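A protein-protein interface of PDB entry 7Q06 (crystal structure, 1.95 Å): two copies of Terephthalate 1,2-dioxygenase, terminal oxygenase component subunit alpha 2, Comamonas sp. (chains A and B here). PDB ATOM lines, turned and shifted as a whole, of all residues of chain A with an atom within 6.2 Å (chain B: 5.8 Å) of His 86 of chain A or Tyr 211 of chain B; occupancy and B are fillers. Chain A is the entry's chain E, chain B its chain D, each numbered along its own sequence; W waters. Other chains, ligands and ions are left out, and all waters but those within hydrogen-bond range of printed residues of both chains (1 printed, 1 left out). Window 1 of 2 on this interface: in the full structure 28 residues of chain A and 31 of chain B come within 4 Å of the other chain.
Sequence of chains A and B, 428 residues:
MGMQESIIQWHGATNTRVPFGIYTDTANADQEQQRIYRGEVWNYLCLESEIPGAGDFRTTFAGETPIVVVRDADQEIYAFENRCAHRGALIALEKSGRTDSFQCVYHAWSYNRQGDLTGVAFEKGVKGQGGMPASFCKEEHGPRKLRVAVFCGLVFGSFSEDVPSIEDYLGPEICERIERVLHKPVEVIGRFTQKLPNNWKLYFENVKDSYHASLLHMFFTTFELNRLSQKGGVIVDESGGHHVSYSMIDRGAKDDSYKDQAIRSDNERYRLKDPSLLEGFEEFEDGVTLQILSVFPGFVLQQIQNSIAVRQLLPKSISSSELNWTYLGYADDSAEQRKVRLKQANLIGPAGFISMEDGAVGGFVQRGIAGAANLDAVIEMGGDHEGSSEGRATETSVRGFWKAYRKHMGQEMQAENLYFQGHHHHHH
Water W1 lies within hydrogen-bond range of the side-chain carboxylate of Glu 395 of chain B (2.7 Å), the backbone carbonyl oxygen of Val 378 of chain B (2.8 Å) and a ring nitrogen (NE2) of His 86 of chain A (3.4 Å).
Among the printed residues, pairs that only touch across the chains: Phe 122 of chain A with Leu 228 of chain B, His 107 of chain A with His 212 of chain B, Phe 122 of chain A with Met 381 of chain B, Arg 87 of chain A with Phe 20 of chain B, His 107 of chain A with Leu 215 of chain B, Tyr 106 of chain A with His 212 of chain B, His 86 of chain A with Ala 377 of chain B, His 107 of chain A with Tyr 211 of chain B, Val 120 of chain A with Tyr 211 of chain B, Phe 122 of chain A with Leu 215 of chain B, Ala 85 of chain A with Val 378 of chain B, Ala 121 of chain A with Leu 215 of chain B, His 86 of chain A with Tyr 211 of chain B, Arg 87 of chain A with Glu 395 of chain B, Tyr 106 of chain A with Asp 209 of chain B, Tyr 106 of chain A with Leu 215 of chain B and Gly 88 of chain A with Phe 20 of chain B.
The guanidinium group (NH1) of Arg 87 of chain A is in salt-bridge range of the side-chain carboxylate (OD2) of Asp 209 of chain B (3.1 Å). A ring nitrogen (NE2) of His 107 of chain A lies within hydrogen-bond range of the side-chain carboxylate (OD2) of Asp 209 of chain B (2.6 Å). OH of Tyr 211 of chain B is in hydrogen-bond range of NE1 of Trp 109 of chain A (2.9 Å). The side-chain hydroxyl (OH) of Tyr 211 of chain B sits at hydrogen-bond distance from the backbone carbonyl oxygen (O) of Ala 121 of chain A, 2.6 Å away. O of His 86 of chain A lies within hydrogen-bond range of N of Val 378 of chain B (2.9 Å). OE2 of Glu 395 of chain B sits at hydrogen-bond distance from NE2 of His 86 of chain A (2.6 Å). The side-chain sulfur (SD) of Met 132 of chain A lies close to the side-chain sulfur (SD) of Met 381 of chain B (3.6 Å).
The backbone carbonyl oxygen (O) of Asp 209 of chain B sits at hydrogen-bond distance from a ring nitrogen (ND1) of His 212 of chain B, at 2.6 Å. N of Tyr 211 of chain B sits at hydrogen-bond distance from O of Arg 392 of chain B (3.3 Å). The side-chain sulfur (SG) of Cys 84 of chain A lies close to the backbone NH (N) of His 86 of chain A, 3.6 Å away.
Cys 84 of chain A touches none of the printed residues of chain B. Of chain B, only Tyr 211, Ala 377, Val 378 and Glu 395 come within 4 Å of His 86 of chain A. Of the printed residues of chain B, Trp 109 of chain A touches Tyr 211 (2.9 Å). Of the printed residues of chain A, Val 378 of chain B touches Ala 85 (3.8 Å) and His 86 (2.9 Å). The nearest residue of chain B that does not touch His 86 of chain A is Asp 376 of chain B (4.7 Å). The nearest printed residue of chain B that does not touch Val 120 of chain A is Met 381 of chain B (5.0 Å).
No position is printed for both chains.
Among the printed residues, 24 pairs touch across the chains. Among the printed residues, Asp or Glu carboxylates within 4 Å of a Lys or Arg side-chain nitrogen of the other chain: Arg 87 of chain A with Asp 209 of chain B (3.1 Å).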
ATOM      1  N   ARG A  83      -1.888   0.831  -2.903  1.00  0.00           N
ATOM      2  CA  ARG A  83      -0.686  -0.022  -2.683  1.00  0.00           C
ATOM      3  C   ARG A  83      -0.980  -0.900  -1.463  1.00  0.00           C
ATOM      4  O   ARG A  83      -1.134  -0.381  -0.362  1.00  0.00           O
ATOM      5  CB  ARG A  83       0.603   0.787  -2.474  1.00  0.00           C
ATOM      6  CG  ARG A  83       1.814  -0.066  -2.152  1.00  0.00           C
ATOM      7  CD  ARG A  83       3.140   0.672  -1.920  1.00  0.00           C
ATOM      8  NE  ARG A  83       2.966   1.796  -1.010  1.00  0.00           N
ATOM      9  CZ  ARG A  83       3.027   1.717   0.321  1.00  0.00           C
ATOM     10  NH1 ARG A  83       2.746   2.751   1.066  1.00  0.00           N
ATOM     11  NH2 ARG A  83       3.307   0.599   0.931  1.00  0.00           N
ATOM     12  N   CYS A  84      -1.064  -2.202  -1.680  1.00  0.00           N
ATOM     13  CA  CYS A  84      -1.301  -3.179  -0.594  1.00  0.00           C
ATOM     14  C   CYS A  84      -0.080  -3.170   0.338  1.00  0.00           C
ATOM     15  O   CYS A  84       1.053  -3.172  -0.141  1.00  0.00           O
ATOM     16  CB  CYS A  84      -1.565  -4.546  -1.182  1.00  0.00           C
ATOM     17  SG  CYS A  84      -1.823  -5.812   0.090  1.00  0.00           S
ATOM     18  N   ALA A  85      -0.325  -3.179   1.639  1.00  0.00           N
ATOM     19  CA  ALA A  85       0.732  -3.038   2.681  1.00  0.00           C
ATOM     20  C   ALA A  85       1.492  -4.357   2.850  1.00  0.00           C
ATOM     21  O   ALA A  85       2.485  -4.381   3.587  1.00  0.00           O
ATOM     22  CB  ALA A  85       0.118  -2.568   3.981  1.00  0.00           C
ATOM     23  N   HIS A  86       1.089  -5.401   2.136  1.00  0.00           N
ATOM     24  CA  HIS A  86       1.774  -6.714   2.147  1.00  0.00           C
ATOM     25  C   HIS A  86       3.020  -6.655   1.244  1.00  0.00           C
ATOM     26  O   HIS A  86       4.156  -6.339   1.762  1.00  0.00           O
ATOM     27  CB  HIS A  86       0.773  -7.832   1.801  1.00  0.00           C
ATOM     28  CG  HIS A  86       1.385  -9.193   1.770  1.00  0.00           C
ATOM     29  ND1 HIS A  86       0.993 -10.161   0.903  1.00  0.00           N
ATOM     30  CD2 HIS A  86       2.345  -9.760   2.542  1.00  0.00           C
ATOM     31  CE1 HIS A  86       1.694 -11.271   1.119  1.00  0.00           C
ATOM     32  NE2 HIS A  86       2.566 -11.036   2.072  1.00  0.00           N
ATOM     33  N   ARG A  87       2.847  -6.962  -0.051  1.00  0.00           N
ATOM     34  CA  ARG A  87       3.946  -7.046  -1.055  1.00  0.00           C
ATOM     35  C   ARG A  87       3.773  -5.971  -2.144  1.00  0.00           C
ATOM     36  O   ARG A  87       4.585  -5.941  -3.059  1.00  0.00           O
ATOM     37  CB  ARG A  87       4.044  -8.503  -1.522  1.00  0.00           C
ATOM     38  CG  ARG A  87       4.556  -9.418  -0.401  1.00  0.00           C
ATOM     39  CD  ARG A  87       5.086 -10.828  -0.674  1.00  0.00           C
ATOM     40  NE  ARG A  87       5.853 -10.676  -1.872  1.00  0.00           N
ATOM     41  CZ  ARG A  87       5.624 -11.284  -3.054  1.00  0.00           C
ATOM     42  NH1 ARG A  87       4.765 -12.308  -3.126  1.00  0.00           N
ATOM     43  NH2 ARG A  87       6.289 -10.810  -4.143  1.00  0.00           N
ATOM     44  N   GLY A  88       2.816  -5.043  -1.997  1.00  0.00           N
ATOM     45  CA  GLY A  88       2.792  -3.770  -2.760  1.00  0.00           C
ATOM     46  C   GLY A  88       1.882  -3.791  -3.998  1.00  0.00           C
ATOM     47  O   GLY A  88       1.889  -2.801  -4.749  1.00  0.00           O
ATOM     48  N   ALA A  89       1.083  -4.829  -4.204  1.00  0.00           N
ATOM     49  CA  ALA A  89       0.117  -4.879  -5.320  1.00  0.00           C
ATOM     50  C   ALA A  89      -0.862  -3.707  -5.297  1.00  0.00           C
ATOM     51  O   ALA A  89      -1.323  -3.289  -4.215  1.00  0.00           O
ATOM     52  CB  ALA A  89      -0.637  -6.198  -5.297  1.00  0.00           C
ATOM     53  N   TYR A 106      -4.076 -10.585  -4.466  1.00  0.00           N
ATOM     54  CA  TYR A 106      -2.878 -11.477  -4.442  1.00  0.00           C
ATOM     55  C   TYR A 106      -2.975 -12.447  -3.232  1.00  0.00           C
ATOM     56  O   TYR A 106      -2.872 -13.643  -3.431  1.00  0.00           O
ATOM     57  CB  TYR A 106      -1.629 -10.613  -4.441  1.00  0.00           C
ATOM     58  CG  TYR A 106      -0.353 -11.270  -4.864  1.00  0.00           C
ATOM     59  CD1 TYR A 106      -0.263 -12.616  -5.160  1.00  0.00           C
ATOM     60  CD2 TYR A 106       0.781 -10.502  -4.996  1.00  0.00           C
ATOM     61  CE1 TYR A 106       0.940 -13.194  -5.538  1.00  0.00           C
ATOM     62  CE2 TYR A 106       1.982 -11.056  -5.393  1.00  0.00           C
ATOM     63  CZ  TYR A 106       2.080 -12.412  -5.656  1.00  0.00           C
ATOM     64  OH  TYR A 106       3.293 -12.899  -6.087  1.00  0.00           O
ATOM     65  N   HIS A 107      -3.161 -11.942  -2.008  1.00  0.00           N
ATOM     66  CA  HIS A 107      -3.304 -12.773  -0.784  1.00  0.00           C
ATOM     67  C   HIS A 107      -4.468 -12.307   0.057  1.00  0.00           C
ATOM     68  O   HIS A 107      -4.501 -12.638   1.284  1.00  0.00           O
ATOM     69  CB  HIS A 107      -2.010 -12.878   0.056  1.00  0.00           C
ATOM     70  CG  HIS A 107      -0.747 -12.893  -0.730  1.00  0.00           C
ATOM     71  ND1 HIS A 107      -0.192 -11.720  -1.290  1.00  0.00           N
ATOM     72  CD2 HIS A 107       0.076 -13.908  -1.084  1.00  0.00           C
ATOM     73  CE1 HIS A 107       0.919 -12.037  -1.923  1.00  0.00           C
ATOM     74  NE2 HIS A 107       1.106 -13.356  -1.828  1.00  0.00           N
ATOM     75  N   ALA A 108      -5.443 -11.668  -0.571  1.00  0.00           N
ATOM     76  CA  ALA A 108      -6.779 -11.409   0.016  1.00  0.00           C
ATOM     77  C   ALA A 108      -6.663 -10.594   1.294  1.00  0.00           C
ATOM     78  O   ALA A 108      -7.396 -10.877   2.219  1.00  0.00           O
ATOM     79  CB  ALA A 108      -7.494 -12.718   0.260  1.00  0.00           C
ATOM     80  N   TRP A 109      -5.740  -9.629   1.395  1.00  0.00           N
ATOM     81  CA  TRP A 109      -5.828  -8.651   2.509  1.00  0.00           C
ATOM     82  C   TRP A 109      -6.988  -7.701   2.199  1.00  0.00           C
ATOM     83  O   TRP A 109      -7.123  -7.290   1.010  1.00  0.00           O
ATOM     84  CB  TRP A 109      -4.504  -7.894   2.720  1.00  0.00           C
ATOM     85  CG  TRP A 109      -3.398  -8.732   3.279  1.00  0.00           C
ATOM     86  CD1 TRP A 109      -3.307 -10.092   3.218  1.00  0.00           C
ATOM     87  CD2 TRP A 109      -2.248  -8.283   4.013  1.00  0.00           C
ATOM     88  NE1 TRP A 109      -2.141 -10.502   3.797  1.00  0.00           N
ATOM     89  CE2 TRP A 109      -1.452  -9.419   4.268  1.00  0.00           C
ATOM     90  CE3 TRP A 109      -1.760  -7.035   4.398  1.00  0.00           C
ATOM     91  CZ2 TRP A 109      -0.240  -9.365   4.961  1.00  0.00           C
ATOM     92  CZ3 TRP A 109      -0.547  -6.972   5.064  1.00  0.00           C
ATOM     93  CH2 TRP A 109       0.186  -8.123   5.380  1.00  0.00           C
ATOM     94  N   TYR A 111      -9.180  -3.995   3.084  1.00  0.00           N
ATOM     95  CA  TYR A 111      -9.040  -2.564   3.480  1.00  0.00           C
ATOM     96  C   TYR A 111     -10.427  -1.942   3.509  1.00  0.00           C
ATOM     97  O   TYR A 111     -11.263  -2.286   2.637  1.00  0.00           O
ATOM     98  CB  TYR A 111      -8.125  -1.836   2.488  1.00  0.00           C
ATOM     99  CG  TYR A 111      -6.734  -2.427   2.433  1.00  0.00           C
ATOM    100  CD1 TYR A 111      -6.447  -3.506   1.600  1.00  0.00           C
ATOM    101  CD2 TYR A 111      -5.719  -1.961   3.277  1.00  0.00           C
ATOM    102  CE1 TYR A 111      -5.201  -4.106   1.598  1.00  0.00           C
ATOM    103  CE2 TYR A 111      -4.451  -2.532   3.232  1.00  0.00           C
ATOM    104  CZ  TYR A 111      -4.201  -3.626   2.421  1.00  0.00           C
ATOM    105  OH  TYR A 111      -2.957  -4.205   2.379  1.00  0.00           O
ATOM    106  N   VAL A 120      -6.354  -9.855   7.271  1.00  0.00           N
ATOM    107  CA  VAL A 120      -5.148 -10.521   6.709  1.00  0.00           C
ATOM    108  C   VAL A 120      -5.499 -11.997   6.556  1.00  0.00           C
ATOM    109  O   VAL A 120      -5.783 -12.612   7.620  1.00  0.00           O
ATOM    110  CB  VAL A 120      -3.930 -10.304   7.618  1.00  0.00           C
ATOM    111  CG1 VAL A 120      -2.782 -11.237   7.217  1.00  0.00           C
ATOM    112  CG2 VAL A 120      -3.499  -8.837   7.624  1.00  0.00           C
ATOM    113  N   ALA A 121      -5.479 -12.542   5.332  1.00  0.00           N
ATOM    114  CA  ALA A 121      -5.898 -13.942   5.116  1.00  0.00           C
ATOM    115  C   ALA A 121      -4.978 -14.870   5.928  1.00  0.00           C
ATOM    116  O   ALA A 121      -3.744 -14.733   5.792  1.00  0.00           O
ATOM    117  CB  ALA A 121      -5.901 -14.292   3.645  1.00  0.00           C
ATOM    118  N   PHE A 122      -5.549 -15.758   6.745  1.00  0.00           N
ATOM    119  CA  PHE A 122      -4.794 -16.787   7.513  1.00  0.00           C
ATOM    120  C   PHE A 122      -3.775 -16.125   8.436  1.00  0.00           C
ATOM    121  O   PHE A 122      -2.697 -16.678   8.671  1.00  0.00           O
ATOM    122  CB  PHE A 122      -4.176 -17.759   6.517  1.00  0.00           C
ATOM    123  CG  PHE A 122      -5.253 -18.505   5.769  1.00  0.00           C
ATOM    124  CD1 PHE A 122      -6.287 -19.118   6.482  1.00  0.00           C
ATOM    125  CD2 PHE A 122      -5.287 -18.561   4.392  1.00  0.00           C
ATOM    126  CE1 PHE A 122      -7.310 -19.793   5.826  1.00  0.00           C
ATOM    127  CE2 PHE A 122      -6.333 -19.189   3.731  1.00  0.00           C
ATOM    128  CZ  PHE A 122      -7.334 -19.820   4.443  1.00  0.00           C
ATOM    129  N   GLU A 123      -4.108 -14.939   8.918  1.00  0.00           N
ATOM    130  CA  GLU A 123      -3.272 -14.184   9.884  1.00  0.00           C
ATOM    131  C   GLU A 123      -2.874 -15.095  11.059  1.00  0.00           C
ATOM    132  O   GLU A 123      -1.740 -14.960  11.546  1.00  0.00           O
ATOM    133  CB  GLU A 123      -4.061 -13.009  10.468  1.00  0.00           C
ATOM    134  CG  GLU A 123      -3.182 -12.091  11.297  1.00  0.00           C
ATOM    135  CD  GLU A 123      -3.872 -10.942  11.985  1.00  0.00           C
ATOM    136  OE1 GLU A 123      -5.004 -10.613  11.602  1.00  0.00           O
ATOM    137  OE2 GLU A 123      -3.236 -10.383  12.891  1.00  0.00           O
ATOM    138  N   MET A 132       0.997 -15.135  11.076  1.00  0.00           N
ATOM    139  CA  MET A 132       1.871 -14.011  11.474  1.00  0.00           C
ATOM    140  C   MET A 132       2.402 -14.298  12.874  1.00  0.00           C
ATOM    141  O   MET A 132       1.749 -14.994  13.634  1.00  0.00           O
ATOM    142  CB  MET A 132       1.041 -12.730  11.479  1.00  0.00           C
ATOM    143  CG  MET A 132       0.640 -12.299  10.048  1.00  0.00           C
ATOM    144  SD  MET A 132       2.060 -12.092   8.984  1.00  0.00           S
ATOM    145  CE  MET A 132       1.247 -11.238   7.614  1.00  0.00           C
ATOM    146  N   PHE B  20      11.810  -2.271  -1.771  1.00  0.00           N
ATOM    147  CA  PHE B  20      11.103  -2.261  -3.082  1.00  0.00           C
ATOM    148  C   PHE B  20      12.037  -1.767  -4.189  1.00  0.00           C
ATOM    149  O   PHE B  20      11.819  -2.057  -5.355  1.00  0.00           O
ATOM    150  CB  PHE B  20       9.837  -1.427  -3.018  1.00  0.00           C
ATOM    151  CG  PHE B  20       8.679  -2.086  -2.318  1.00  0.00           C
ATOM    152  CD1 PHE B  20       8.281  -3.370  -2.659  1.00  0.00           C
ATOM    153  CD2 PHE B  20       7.916  -1.374  -1.413  1.00  0.00           C
ATOM    154  CE1 PHE B  20       7.162  -3.947  -2.081  1.00  0.00           C
ATOM    155  CE2 PHE B  20       6.783  -1.937  -0.849  1.00  0.00           C
ATOM    156  CZ  PHE B  20       6.406  -3.231  -1.178  1.00  0.00           C
ATOM    157  N   LYS B 208       7.249 -19.402  -5.703  1.00  0.00           N
ATOM    158  CA  LYS B 208       7.623 -19.866  -4.335  1.00  0.00           C
ATOM    159  C   LYS B 208       6.531 -19.506  -3.327  1.00  0.00           C
ATOM    160  O   LYS B 208       6.697 -19.872  -2.136  1.00  0.00           O
ATOM    161  CB  LYS B 208       8.972 -19.243  -3.957  1.00  0.00           C
ATOM    162  CG  LYS B 208      10.136 -19.725  -4.807  1.00  0.00           C
ATOM    163  CD  LYS B 208      11.405 -18.974  -4.604  1.00  0.00           C
ATOM    164  CE  LYS B 208      12.566 -19.519  -5.405  1.00  0.00           C
ATOM    165  NZ  LYS B 208      12.951 -20.876  -4.958  1.00  0.00           N
ATOM    166  N   ASP B 209       5.478 -18.803  -3.741  1.00  0.00           N
ATOM    167  CA  ASP B 209       4.555 -18.188  -2.767  1.00  0.00           C
ATOM    168  C   ASP B 209       3.425 -19.173  -2.501  1.00  0.00           C
ATOM    169  O   ASP B 209       2.385 -19.065  -3.160  1.00  0.00           O
ATOM    170  CB  ASP B 209       4.156 -16.786  -3.252  1.00  0.00           C
ATOM    171  CG  ASP B 209       3.280 -15.974  -2.316  1.00  0.00           C
ATOM    172  OD1 ASP B 209       2.781 -16.529  -1.311  1.00  0.00           O
ATOM    173  OD2 ASP B 209       3.045 -14.823  -2.643  1.00  0.00           O
ATOM    174  N   SER B 210       3.609 -20.078  -1.524  1.00  0.00           N
ATOM    175  CA  SER B 210       2.588 -21.105  -1.155  1.00  0.00           C
ATOM    176  C   SER B 210       1.377 -20.385  -0.599  1.00  0.00           C
ATOM    177  O   SER B 210       0.256 -20.847  -0.839  1.00  0.00           O
ATOM    178  CB  SER B 210       3.147 -22.129  -0.191  1.00  0.00           C
ATOM    179  OG  SER B 210       3.715 -21.499   0.989  1.00  0.00           O
ATOM    180  N   TYR B 211       1.601 -19.269   0.107  1.00  0.00           N
ATOM    181  CA  TYR B 211       0.517 -18.440   0.711  1.00  0.00           C
ATOM    182  C   TYR B 211      -0.508 -18.068  -0.366  1.00  0.00           C
ATOM    183  O   TYR B 211      -1.725 -18.263  -0.149  1.00  0.00           O
ATOM    184  CB  TYR B 211       1.131 -17.252   1.446  1.00  0.00           C
ATOM    185  CG  TYR B 211       0.217 -16.277   2.137  1.00  0.00           C
ATOM    186  CD1 TYR B 211      -1.024 -16.619   2.646  1.00  0.00           C
ATOM    187  CD2 TYR B 211       0.688 -14.992   2.412  1.00  0.00           C
ATOM    188  CE1 TYR B 211      -1.813 -15.682   3.320  1.00  0.00           C
ATOM    189  CE2 TYR B 211      -0.074 -14.059   3.109  1.00  0.00           C
ATOM    190  CZ  TYR B 211      -1.341 -14.390   3.570  1.00  0.00           C
ATOM    191  OH  TYR B 211      -2.031 -13.405   4.271  1.00  0.00           O
ATOM    192  N   HIS B 212      -0.067 -17.525  -1.503  1.00  0.00           N
ATOM    193  CA  HIS B 212      -1.014 -16.973  -2.510  1.00  0.00           C
ATOM    194  C   HIS B 212      -1.825 -18.071  -3.213  1.00  0.00           C
ATOM    195  O   HIS B 212      -2.901 -17.723  -3.689  1.00  0.00           O
ATOM    196  CB  HIS B 212      -0.300 -16.050  -3.529  1.00  0.00           C
ATOM    197  CG  HIS B 212       0.064 -16.704  -4.796  1.00  0.00           C
ATOM    198  ND1 HIS B 212       1.207 -17.494  -4.902  1.00  0.00           N
ATOM    199  CD2 HIS B 212      -0.540 -16.679  -6.016  1.00  0.00           C
ATOM    200  CE1 HIS B 212       1.294 -17.971  -6.139  1.00  0.00           C
ATOM    201  NE2 HIS B 212       0.215 -17.459  -6.855  1.00  0.00           N
ATOM    202  N   ALA B 213      -1.344 -19.309  -3.368  1.00  0.00           N
ATOM    203  CA  ALA B 213      -1.908 -20.276  -4.349  1.00  0.00           C
ATOM    204  C   ALA B 213      -3.446 -20.409  -4.256  1.00  0.00           C
ATOM    205  O   ALA B 213      -4.141 -20.359  -5.299  1.00  0.00           O
ATOM    206  CB  ALA B 213      -1.229 -21.606  -4.205  1.00  0.00           C
ATOM    207  N   SER B 214      -3.986 -20.524  -3.054  1.00  0.00           N
ATOM    208  CA  SER B 214      -5.430 -20.736  -2.783  1.00  0.00           C
ATOM    209  C   SER B 214      -6.195 -19.416  -2.741  1.00  0.00           C
ATOM    210  O   SER B 214      -7.442 -19.468  -2.760  1.00  0.00           O
ATOM    211  CB  SER B 214      -5.603 -21.495  -1.459  1.00  0.00           C
ATOM    212  OG  SER B 214      -5.126 -20.705  -0.373  1.00  0.00           O
ATOM    213  N   LEU B 215      -5.498 -18.267  -2.722  1.00  0.00           N
ATOM    214  CA  LEU B 215      -6.090 -16.914  -2.474  1.00  0.00           C
ATOM    215  C   LEU B 215      -6.243 -16.115  -3.785  1.00  0.00           C
ATOM    216  O   LEU B 215      -7.373 -15.649  -4.098  1.00  0.00           O
ATOM    217  CB  LEU B 215      -5.193 -16.179  -1.480  1.00  0.00           C
ATOM    218  CG  LEU B 215      -5.036 -16.869  -0.124  1.00  0.00           C
ATOM    219  CD1 LEU B 215      -4.107 -16.049   0.739  1.00  0.00           C
ATOM    220  CD2 LEU B 215      -6.378 -17.085   0.587  1.00  0.00           C
ATOM    221  N   LEU B 228      -5.157 -24.694   1.615  1.00  0.00           N
ATOM    222  CA  LEU B 228      -4.136 -24.698   2.705  1.00  0.00           C
ATOM    223  C   LEU B 228      -4.446 -25.797   3.737  1.00  0.00           C
ATOM    224  O   LEU B 228      -3.499 -26.232   4.389  1.00  0.00           O
ATOM    225  CB  LEU B 228      -4.081 -23.330   3.383  1.00  0.00           C
ATOM    226  CG  LEU B 228      -3.397 -22.220   2.579  1.00  0.00           C
ATOM    227  CD1 LEU B 228      -3.656 -20.863   3.215  1.00  0.00           C
ATOM    228  CD2 LEU B 228      -1.895 -22.462   2.427  1.00  0.00           C
ATOM    229  N   ASP B 376       9.320  -1.040   2.025  1.00  0.00           N
ATOM    230  CA  ASP B 376       9.720  -2.461   2.171  1.00  0.00           C
ATOM    231  C   ASP B 376       8.484  -3.357   2.061  1.00  0.00           C
ATOM    232  O   ASP B 376       7.403  -3.041   2.642  1.00  0.00           O
ATOM    233  CB  ASP B 376      10.398  -2.746   3.531  1.00  0.00           C
ATOM    234  CG  ASP B 376      11.811  -2.196   3.741  1.00  0.00           C
ATOM    235  OD1 ASP B 376      12.471  -1.844   2.771  1.00  0.00           O
ATOM    236  OD2 ASP B 376      12.241  -2.144   4.901  1.00  0.00           O
ATOM    237  N   ALA B 377       8.633  -4.462   1.350  1.00  0.00           N
ATOM    238  CA  ALA B 377       7.675  -5.569   1.395  1.00  0.00           C
ATOM    239  C   ALA B 377       7.716  -6.193   2.796  1.00  0.00           C
ATOM    240  O   ALA B 377       8.804  -6.274   3.392  1.00  0.00           O
ATOM    241  CB  ALA B 377       7.967  -6.567   0.310  1.00  0.00           C
ATOM    242  N   VAL B 378       6.564  -6.648   3.275  1.00  0.00           N
ATOM    243  CA  VAL B 378       6.410  -7.346   4.578  1.00  0.00           C
ATOM    244  C   VAL B 378       6.238  -8.847   4.308  1.00  0.00           C
ATOM    245  O   VAL B 378       5.213  -9.247   3.716  1.00  0.00           O
ATOM    246  CB  VAL B 378       5.222  -6.737   5.346  1.00  0.00           C
ATOM    247  CG1 VAL B 378       4.887  -7.585   6.585  1.00  0.00           C
ATOM    248  CG2 VAL B 378       5.502  -5.296   5.753  1.00  0.00           C
ATOM    249  N   ILE B 379       7.189  -9.661   4.735  1.00  0.00           N
ATOM    250  CA  ILE B 379       7.179 -11.116   4.471  1.00  0.00           C
ATOM    251  C   ILE B 379       7.359 -11.887   5.795  1.00  0.00           C
ATOM    252  O   ILE B 379       8.487 -12.406   6.062  1.00  0.00           O
ATOM    253  CB  ILE B 379       8.292 -11.428   3.475  1.00  0.00           C
ATOM    254  CG1 ILE B 379       8.283 -10.432   2.308  1.00  0.00           C
ATOM    255  CG2 ILE B 379       8.133 -12.879   3.032  1.00  0.00           C
ATOM    256  CD1 ILE B 379       9.234 -10.770   1.195  1.00  0.00           C
ATOM    257  N   MET B 381       4.833 -14.270   7.218  1.00  0.00           N
ATOM    258  CA  MET B 381       4.021 -15.508   7.426  1.00  0.00           C
ATOM    259  C   MET B 381       4.962 -16.684   7.712  1.00  0.00           C
ATOM    260  O   MET B 381       5.923 -16.860   6.951  1.00  0.00           O
ATOM    261  CB  MET B 381       3.142 -15.788   6.199  1.00  0.00           C
ATOM    262  CG  MET B 381       2.058 -14.742   6.021  1.00  0.00           C
ATOM    263  SD  MET B 381       0.689 -14.874   7.210  1.00  0.00           S
ATOM    264  CE  MET B 381      -0.122 -16.341   6.573  1.00  0.00           C
ATOM    265  N   ARG B 392       1.144 -24.540   4.476  1.00  0.00           N
ATOM    266  CA  ARG B 392       1.483 -23.677   3.327  1.00  0.00           C
ATOM    267  C   ARG B 392       1.080 -22.221   3.611  1.00  0.00           C
ATOM    268  O   ARG B 392       1.393 -21.369   2.707  1.00  0.00           O
ATOM    269  CB  ARG B 392       0.856 -24.341   2.098  1.00  0.00           C
ATOM    270  CG  ARG B 392       1.779 -25.395   1.483  1.00  0.00           C
ATOM    271  CD  ARG B 392       1.219 -26.757   1.104  1.00  0.00           C
ATOM    272  NE  ARG B 392      -0.211 -26.805   0.858  1.00  0.00           N
ATOM    273  CZ  ARG B 392      -0.804 -26.785  -0.343  1.00  0.00           C
ATOM    274  NH1 ARG B 392      -0.084 -26.728  -1.467  1.00  0.00           N
ATOM    275  NH2 ARG B 392      -2.131 -26.831  -0.384  1.00  0.00           N
ATOM    276  N   ALA B 393       0.524 -21.920   4.806  1.00  0.00           N
ATOM    277  CA  ALA B 393       0.267 -20.537   5.299  1.00  0.00           C
ATOM    278  C   ALA B 393       1.575 -19.937   5.833  1.00  0.00           C
ATOM    279  O   ALA B 393       1.657 -19.492   7.023  1.00  0.00           O
ATOM    280  CB  ALA B 393      -0.838 -20.534   6.339  1.00  0.00           C
ATOM    281  N   THR B 394       2.593 -19.931   4.976  1.00  0.00           N
ATOM    282  CA  THR B 394       3.961 -19.482   5.271  1.00  0.00           C
ATOM    283  C   THR B 394       4.548 -18.803   4.033  1.00  0.00           C
ATOM    284  O   THR B 394       4.030 -19.051   2.922  1.00  0.00           O
ATOM    285  CB  THR B 394       4.816 -20.681   5.714  1.00  0.00           C
ATOM    286  OG1 THR B 394       6.114 -20.166   6.025  1.00  0.00           O
ATOM    287  CG2 THR B 394       4.896 -21.752   4.648  1.00  0.00           C
ATOM    288  N   GLU B 395       5.604 -18.004   4.237  1.00  0.00           N
ATOM    289  CA  GLU B 395       6.385 -17.360   3.166  1.00  0.00           C
ATOM    290  C   GLU B 395       7.827 -17.836   3.283  1.00  0.00           C
ATOM    291  O   GLU B 395       8.701 -17.168   2.699  1.00  0.00           O
ATOM    292  CB  GLU B 395       6.222 -15.847   3.252  1.00  0.00           C
ATOM    293  CG  GLU B 395       4.849 -15.361   2.747  1.00  0.00           C
ATOM    294  CD  GLU B 395       4.515 -13.941   3.165  1.00  0.00           C
ATOM    295  OE1 GLU B 395       4.720 -13.615   4.370  1.00  0.00           O
ATOM    296  OE2 GLU B 395       4.067 -13.133   2.300  1.00  0.00           O
HETATM  297  O   HOH W   1       3.863 -11.198   5.243  1.00  0.00           O
